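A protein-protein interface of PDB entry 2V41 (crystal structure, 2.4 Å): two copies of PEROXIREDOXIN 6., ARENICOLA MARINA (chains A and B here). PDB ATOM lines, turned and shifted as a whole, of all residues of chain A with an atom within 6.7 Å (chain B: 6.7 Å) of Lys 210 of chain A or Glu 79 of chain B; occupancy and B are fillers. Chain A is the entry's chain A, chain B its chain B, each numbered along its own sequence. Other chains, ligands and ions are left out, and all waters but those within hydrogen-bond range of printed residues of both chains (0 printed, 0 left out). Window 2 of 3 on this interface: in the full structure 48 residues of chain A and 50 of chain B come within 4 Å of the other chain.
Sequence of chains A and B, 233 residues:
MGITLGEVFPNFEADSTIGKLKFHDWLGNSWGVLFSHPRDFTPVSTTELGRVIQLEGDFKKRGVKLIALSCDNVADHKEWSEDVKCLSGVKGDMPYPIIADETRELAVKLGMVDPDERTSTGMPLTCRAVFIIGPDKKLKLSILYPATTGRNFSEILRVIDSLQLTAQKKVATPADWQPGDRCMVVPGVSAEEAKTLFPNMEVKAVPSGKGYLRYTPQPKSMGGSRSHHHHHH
Of the 11 printed residues of chain A, 5 touch a printed residue of chain B. Printed residues of chain A that touch a printed residue of chain B: Val 206, Pro 207, Ser 208, Lys 210 and Tyr 212. Hydrophobic or aromatic side chains of chain A that line the printed part of chain B: Val 206, Pro 207 and Tyr 212. Printed residues of chain B that touch a printed residue of chain A: Phe 41, Glu 79, Trp 80, Glu 82 and Asp 83. Among the printed residues, Asp or Glu carboxylates within 4 Å of a Lys or Arg side-chain nitrogen of the other chain: Lys 210 of chain A with Glu 79 of chain B (3.8 Å).
OG of Ser 208 of chain A sits at hydrogen-bond distance from OD2 of Asp 83 of chain B, at 2.8 Å. NZ of Lys 210 of chain A is in salt-bridge range of OE2 of Glu 79 of chain B. The indole nitrogen (NE1) of Trp 80 of chain B sits at hydrogen-bond distance from the side-chain hydroxyl (OH) of Tyr 212 of chain A (3.3 Å). The side-chain hydroxyl (OH) of Tyr 212 of chain A sits at hydrogen-bond distance from the side-chain carboxylate (OD2) of Asp 83 of chain B, 2.6 Å away.
No position is printed for both chains.
OG of Ser 208 of chain A lies close to N of Lys 210 of chain A (3.3 Å).
Ala 205 of chain A touches none of the printed residues of chain B. Printed residues of chain B within 4 Å of Val 206 of chain A: Asp 83. Of the printed residues of chain B, Pro 207 of chain A touches Glu 82 and Asp 83. Lys 210 of chain A touches just these residues of chain B: Phe 41 and Glu 79. Glu 79 of chain B touches just these residues of chain A: Ser 208 and Lys 210. The nearest residue of chain B that does not touch Lys 210 of chain A is Asp 83 of chain B (5.4 Å). The nearest residue of chain A that does not touch Glu 79 of chain B is Gly 209 of chain A (6.3 Å). The nearest printed residue of chain B that does not touch Ser 208 of chain A is Phe 41 of chain B (4.3 Å).
Asp 83 of chain B touches Val 206 of chain A (OD2 to CG2, 3.3 Å). CG of Pro 207 of chain A touches O of Glu 82 of chain B, 3.6 Å away. Pro 207 of chain A touches Asp 83 of chain B. Ser 208 of chain A touches Glu 79 of chain B. Phe 41 of chain B touches Lys 210 of chain A (CD1 to CE, 3.6 Å). Phe 41 of chain B touches Tyr 212 of chain A (O to CG, 3.4 Å).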
ATOM      1  N   VAL A 203      11.870   0.663 -16.769  1.00  0.00           N
ATOM      2  CA  VAL A 203      11.433  -0.409 -17.648  1.00  0.00           C
ATOM      3  C   VAL A 203      12.446  -1.564 -17.518  1.00  0.00           C
ATOM      4  O   VAL A 203      13.586  -1.416 -17.893  1.00  0.00           O
ATOM      5  CB  VAL A 203      11.348   0.071 -19.117  1.00  0.00           C
ATOM      6  CG1 VAL A 203      10.629  -1.001 -19.977  1.00  0.00           C
ATOM      7  CG2 VAL A 203      10.630   1.512 -19.231  1.00  0.00           C
ATOM      8  N   LYS A 204      12.026  -2.698 -16.953  1.00  0.00           N
ATOM      9  CA  LYS A 204      12.898  -3.857 -16.784  1.00  0.00           C
ATOM     10  C   LYS A 204      12.863  -4.816 -17.981  1.00  0.00           C
ATOM     11  O   LYS A 204      11.875  -5.527 -18.228  1.00  0.00           O
ATOM     12  CB  LYS A 204      12.505  -4.625 -15.521  1.00  0.00           C
ATOM     13  CG  LYS A 204      13.592  -5.563 -15.054  1.00  0.00           C
ATOM     14  CD  LYS A 204      13.305  -6.134 -13.702  1.00  0.00           C
ATOM     15  CE  LYS A 204      14.562  -6.728 -13.019  1.00  0.00           C
ATOM     16  NZ  LYS A 204      15.582  -7.426 -13.844  1.00  0.00           N
ATOM     17  N   ALA A 205      13.952  -4.839 -18.715  1.00  0.00           N
ATOM     18  CA  ALA A 205      14.195  -5.831 -19.762  1.00  0.00           C
ATOM     19  C   ALA A 205      13.908  -7.274 -19.310  1.00  0.00           C
ATOM     20  O   ALA A 205      14.450  -7.750 -18.293  1.00  0.00           O
ATOM     21  CB  ALA A 205      15.668  -5.711 -20.260  1.00  0.00           C
ATOM     22  N   VAL A 206      13.077  -7.945 -20.113  1.00  0.00           N
ATOM     23  CA  VAL A 206      12.749  -9.375 -19.978  1.00  0.00           C
ATOM     24  C   VAL A 206      13.118 -10.128 -21.265  1.00  0.00           C
ATOM     25  O   VAL A 206      13.161  -9.529 -22.345  1.00  0.00           O
ATOM     26  CB  VAL A 206      11.244  -9.565 -19.671  1.00  0.00           C
ATOM     27  CG1 VAL A 206      10.931  -9.078 -18.297  1.00  0.00           C
ATOM     28  CG2 VAL A 206      10.379  -8.812 -20.666  1.00  0.00           C
ATOM     29  N   PRO A 207      13.371 -11.453 -21.173  1.00  0.00           N
ATOM     30  CA  PRO A 207      13.766 -12.223 -22.364  1.00  0.00           C
ATOM     31  C   PRO A 207      12.870 -12.048 -23.582  1.00  0.00           C
ATOM     32  O   PRO A 207      13.373 -12.146 -24.701  1.00  0.00           O
ATOM     33  CB  PRO A 207      13.714 -13.674 -21.887  1.00  0.00           C
ATOM     34  CG  PRO A 207      13.961 -13.596 -20.443  1.00  0.00           C
ATOM     35  CD  PRO A 207      13.316 -12.310 -19.975  1.00  0.00           C
ATOM     36  N   SER A 208      11.576 -11.784 -23.384  1.00  0.00           N
ATOM     37  CA  SER A 208      10.610 -11.707 -24.510  1.00  0.00           C
ATOM     38  C   SER A 208      10.734 -10.431 -25.388  1.00  0.00           C
ATOM     39  O   SER A 208      10.138 -10.351 -26.465  1.00  0.00           O
ATOM     40  CB  SER A 208       9.164 -11.854 -23.994  1.00  0.00           C
ATOM     41  OG  SER A 208       8.690 -10.626 -23.512  1.00  0.00           O
ATOM     42  N   GLY A 209      11.501  -9.447 -24.913  1.00  0.00           N
ATOM     43  CA  GLY A 209      11.624  -8.159 -25.565  1.00  0.00           C
ATOM     44  C   GLY A 209      10.447  -7.203 -25.379  1.00  0.00           C
ATOM     45  O   GLY A 209      10.443  -6.112 -25.969  1.00  0.00           O
ATOM     46  N   LYS A 210       9.432  -7.584 -24.606  1.00  0.00           N
ATOM     47  CA  LYS A 210       8.317  -6.662 -24.418  1.00  0.00           C
ATOM     48  C   LYS A 210       8.643  -5.646 -23.285  1.00  0.00           C
ATOM     49  O   LYS A 210       9.597  -5.817 -22.475  1.00  0.00           O
ATOM     50  CB  LYS A 210       7.013  -7.411 -24.197  1.00  0.00           C
ATOM     51  CG  LYS A 210       6.691  -8.477 -25.284  1.00  0.00           C
ATOM     52  CD  LYS A 210       5.181  -8.868 -25.281  1.00  0.00           C
ATOM     53  CE  LYS A 210       4.855 -10.197 -25.958  1.00  0.00           C
ATOM     54  NZ  LYS A 210       5.803 -10.546 -27.046  1.00  0.00           N
ATOM     55  N   GLY A 211       7.867  -4.566 -23.255  1.00  0.00           N
ATOM     56  CA  GLY A 211       8.206  -3.399 -22.428  1.00  0.00           C
ATOM     57  C   GLY A 211       7.166  -3.098 -21.376  1.00  0.00           C
ATOM     58  O   GLY A 211       6.994  -1.941 -20.950  1.00  0.00           O
ATOM     59  N   TYR A 212       6.498  -4.165 -20.960  1.00  0.00           N
ATOM     60  CA  TYR A 212       5.349  -4.116 -19.981  1.00  0.00           C
ATOM     61  C   TYR A 212       5.746  -4.043 -18.498  1.00  0.00           C
ATOM     62  O   TYR A 212       4.966  -3.588 -17.673  1.00  0.00           O
ATOM     63  CB  TYR A 212       4.420  -5.303 -20.224  1.00  0.00           C
ATOM     64  CG  TYR A 212       5.045  -6.655 -19.930  1.00  0.00           C
ATOM     65  CD1 TYR A 212       5.045  -7.183 -18.629  1.00  0.00           C
ATOM     66  CD2 TYR A 212       5.607  -7.420 -20.945  1.00  0.00           C
ATOM     67  CE1 TYR A 212       5.623  -8.419 -18.357  1.00  0.00           C
ATOM     68  CE2 TYR A 212       6.205  -8.641 -20.661  1.00  0.00           C
ATOM     69  CZ  TYR A 212       6.215  -9.135 -19.364  1.00  0.00           C
ATOM     70  OH  TYR A 212       6.787 -10.363 -19.062  1.00  0.00           O
ATOM     71  N   LEU A 213       6.971  -4.473 -18.189  1.00  0.00           N
ATOM     72  CA  LEU A 213       7.463  -4.640 -16.823  1.00  0.00           C
ATOM     73  C   LEU A 213       8.008  -3.271 -16.346  1.00  0.00           C
ATOM     74  O   LEU A 213       9.179  -3.017 -16.318  1.00  0.00           O
ATOM     75  CB  LEU A 213       8.503  -5.787 -16.763  1.00  0.00           C
ATOM     76  CG  LEU A 213       8.821  -6.494 -15.429  1.00  0.00           C
ATOM     77  CD1 LEU A 213       7.553  -6.934 -14.633  1.00  0.00           C
ATOM     78  CD2 LEU A 213       9.696  -7.667 -15.708  1.00  0.00           C
ATOM     79  N   PHE B  41       1.988 -11.561 -20.264  1.00  0.00           N
ATOM     80  CA  PHE B  41       2.787 -10.386 -20.528  1.00  0.00           C
ATOM     81  C   PHE B  41       2.189  -9.158 -19.872  1.00  0.00           C
ATOM     82  O   PHE B  41       2.036  -8.145 -20.506  1.00  0.00           O
ATOM     83  CB  PHE B  41       2.951 -10.180 -22.019  1.00  0.00           C
ATOM     84  CG  PHE B  41       3.365 -11.433 -22.781  1.00  0.00           C
ATOM     85  CD1 PHE B  41       4.679 -11.893 -22.735  1.00  0.00           C
ATOM     86  CD2 PHE B  41       2.442 -12.125 -23.572  1.00  0.00           C
ATOM     87  CE1 PHE B  41       5.076 -13.034 -23.477  1.00  0.00           C
ATOM     88  CE2 PHE B  41       2.813 -13.273 -24.275  1.00  0.00           C
ATOM     89  CZ  PHE B  41       4.131 -13.720 -24.246  1.00  0.00           C
ATOM     90  N   VAL B  74      -1.808 -21.393 -25.085  1.00  0.00           N
ATOM     91  CA  VAL B  74      -0.660 -22.074 -24.483  1.00  0.00           C
ATOM     92  C   VAL B  74       0.673 -21.585 -25.123  1.00  0.00           C
ATOM     93  O   VAL B  74       1.703 -21.533 -24.442  1.00  0.00           O
ATOM     94  CB  VAL B  74      -0.826 -23.629 -24.535  1.00  0.00           C
ATOM     95  CG1 VAL B  74       0.399 -24.309 -24.067  1.00  0.00           C
ATOM     96  CG2 VAL B  74      -1.979 -24.085 -23.651  1.00  0.00           C
ATOM     97  N   ALA B  75       0.664 -21.185 -26.393  1.00  0.00           N
ATOM     98  CA  ALA B  75       1.834 -20.496 -26.968  1.00  0.00           C
ATOM     99  C   ALA B  75       2.251 -19.255 -26.127  1.00  0.00           C
ATOM    100  O   ALA B  75       3.437 -19.048 -25.833  1.00  0.00           O
ATOM    101  CB  ALA B  75       1.555 -20.098 -28.395  1.00  0.00           C
ATOM    102  N   ASP B  76       1.276 -18.452 -25.706  1.00  0.00           N
ATOM    103  CA  ASP B  76       1.573 -17.241 -24.933  1.00  0.00           C
ATOM    104  C   ASP B  76       2.048 -17.624 -23.525  1.00  0.00           C
ATOM    105  O   ASP B  76       2.934 -16.986 -22.957  1.00  0.00           O
ATOM    106  CB  ASP B  76       0.355 -16.292 -24.869  1.00  0.00           C
ATOM    107  CG  ASP B  76       0.081 -15.521 -26.199  1.00  0.00           C
ATOM    108  OD1 ASP B  76       0.909 -15.488 -27.154  1.00  0.00           O
ATOM    109  OD2 ASP B  76      -1.017 -14.934 -26.293  1.00  0.00           O
ATOM    110  N   HIS B  77       1.474 -18.671 -22.954  1.00  0.00           N
ATOM    111  CA  HIS B  77       1.944 -19.178 -21.653  1.00  0.00           C
ATOM    112  C   HIS B  77       3.412 -19.671 -21.673  1.00  0.00           C
ATOM    113  O   HIS B  77       4.169 -19.404 -20.730  1.00  0.00           O
ATOM    114  CB  HIS B  77       1.050 -20.314 -21.173  1.00  0.00           C
ATOM    115  CG  HIS B  77      -0.295 -19.875 -20.704  1.00  0.00           C
ATOM    116  ND1 HIS B  77      -1.304 -20.766 -20.406  1.00  0.00           N
ATOM    117  CD2 HIS B  77      -0.803 -18.646 -20.473  1.00  0.00           C
ATOM    118  CE1 HIS B  77      -2.369 -20.099 -20.001  1.00  0.00           C
ATOM    119  NE2 HIS B  77      -2.097 -18.813 -20.038  1.00  0.00           N
ATOM    120  N   LYS B  78       3.810 -20.387 -22.728  1.00  0.00           N
ATOM    121  CA  LYS B  78       5.184 -20.882 -22.821  1.00  0.00           C
ATOM    122  C   LYS B  78       6.199 -19.718 -22.957  1.00  0.00           C
ATOM    123  O   LYS B  78       7.177 -19.633 -22.201  1.00  0.00           O
ATOM    124  CB  LYS B  78       5.336 -21.871 -23.974  1.00  0.00           C
ATOM    125  CG  LYS B  78       4.733 -23.268 -23.712  1.00  0.00           C
ATOM    126  CD  LYS B  78       4.929 -24.159 -24.968  1.00  0.00           C
ATOM    127  CE  LYS B  78       3.852 -25.312 -25.129  1.00  0.00           C
ATOM    128  NZ  LYS B  78       3.950 -26.084 -26.467  1.00  0.00           N
ATOM    129  N   GLU B  79       5.951 -18.817 -23.904  1.00  0.00           N
ATOM    130  CA  GLU B  79       6.835 -17.666 -24.109  1.00  0.00           C
ATOM    131  C   GLU B  79       6.944 -16.839 -22.833  1.00  0.00           C
ATOM    132  O   GLU B  79       8.042 -16.589 -22.351  1.00  0.00           O
ATOM    133  CB  GLU B  79       6.348 -16.796 -25.265  1.00  0.00           C
ATOM    134  CG  GLU B  79       7.431 -15.983 -25.908  1.00  0.00           C
ATOM    135  CD  GLU B  79       6.882 -14.895 -26.792  1.00  0.00           C
ATOM    136  OE1 GLU B  79       5.742 -15.055 -27.261  1.00  0.00           O
ATOM    137  OE2 GLU B  79       7.580 -13.885 -27.006  1.00  0.00           O
ATOM    138  N   TRP B  80       5.798 -16.493 -22.250  1.00  0.00           N
ATOM    139  CA  TRP B  80       5.753 -15.584 -21.114  1.00  0.00           C
ATOM    140  C   TRP B  80       6.421 -16.141 -19.851  1.00  0.00           C
ATOM    141  O   TRP B  80       6.987 -15.389 -19.080  1.00  0.00           O
ATOM    142  CB  TRP B  80       4.314 -15.170 -20.808  1.00  0.00           C
ATOM    143  CG  TRP B  80       4.202 -14.273 -19.617  1.00  0.00           C
ATOM    144  CD1 TRP B  80       4.873 -13.105 -19.403  1.00  0.00           C
ATOM    145  CD2 TRP B  80       3.346 -14.460 -18.482  1.00  0.00           C
ATOM    146  NE1 TRP B  80       4.501 -12.564 -18.189  1.00  0.00           N
ATOM    147  CE2 TRP B  80       3.551 -13.377 -17.620  1.00  0.00           C
ATOM    148  CE3 TRP B  80       2.452 -15.459 -18.101  1.00  0.00           C
ATOM    149  CZ2 TRP B  80       2.889 -13.256 -16.446  1.00  0.00           C
ATOM    150  CZ3 TRP B  80       1.785 -15.323 -16.924  1.00  0.00           C
ATOM    151  CH2 TRP B  80       2.016 -14.243 -16.106  1.00  0.00           C
ATOM    152  N   SER B  81       6.341 -17.458 -19.666  1.00  0.00           N
ATOM    153  CA  SER B  81       7.051 -18.134 -18.580  1.00  0.00           C
ATOM    154  C   SER B  81       8.507 -17.801 -18.581  1.00  0.00           C
ATOM    155  O   SER B  81       9.072 -17.649 -17.543  1.00  0.00           O
ATOM    156  CB  SER B  81       6.865 -19.633 -18.652  1.00  0.00           C
ATOM    157  OG  SER B  81       5.484 -19.966 -18.605  1.00  0.00           O
ATOM    158  N   GLU B  82       9.119 -17.634 -19.755  1.00  0.00           N
ATOM    159  CA  GLU B  82      10.525 -17.275 -19.795  1.00  0.00           C
ATOM    160  C   GLU B  82      10.745 -15.907 -19.121  1.00  0.00           C
ATOM    161  O   GLU B  82      11.782 -15.686 -18.508  1.00  0.00           O
ATOM    162  CB  GLU B  82      11.058 -17.300 -21.217  1.00  0.00           C
ATOM    163  CG  GLU B  82      11.068 -18.677 -21.850  1.00  0.00           C
ATOM    164  CD  GLU B  82      11.848 -19.714 -21.048  1.00  0.00           C
ATOM    165  OE1 GLU B  82      13.067 -19.555 -20.905  1.00  0.00           O
ATOM    166  OE2 GLU B  82      11.255 -20.695 -20.564  1.00  0.00           O
ATOM    167  N   ASP B  83       9.778 -15.002 -19.196  1.00  0.00           N
ATOM    168  CA  ASP B  83       9.884 -13.738 -18.434  1.00  0.00           C
ATOM    169  C   ASP B  83       9.645 -13.932 -16.940  1.00  0.00           C
ATOM    170  O   ASP B  83      10.250 -13.278 -16.101  1.00  0.00           O
ATOM    171  CB  ASP B  83       8.877 -12.707 -18.939  1.00  0.00           C
ATOM    172  CG  ASP B  83       9.137 -12.282 -20.352  1.00  0.00           C
ATOM    173  OD1 ASP B  83      10.107 -12.793 -20.987  1.00  0.00           O
ATOM    174  OD2 ASP B  83       8.347 -11.424 -20.819  1.00  0.00           O
ATOM    175  N   VAL B  84       8.697 -14.812 -16.624  1.00  0.00           N
ATOM    176  CA  VAL B  84       8.322 -15.088 -15.268  1.00  0.00           C
ATOM    177  C   VAL B  84       9.526 -15.702 -14.527  1.00  0.00           C
ATOM    178  O   VAL B  84       9.888 -15.232 -13.450  1.00  0.00           O
ATOM    179  CB  VAL B  84       7.024 -15.948 -15.212  1.00  0.00           C
ATOM    180  CG1 VAL B  84       6.645 -16.299 -13.745  1.00  0.00           C
ATOM    181  CG2 VAL B  84       5.859 -15.168 -15.873  1.00  0.00           C
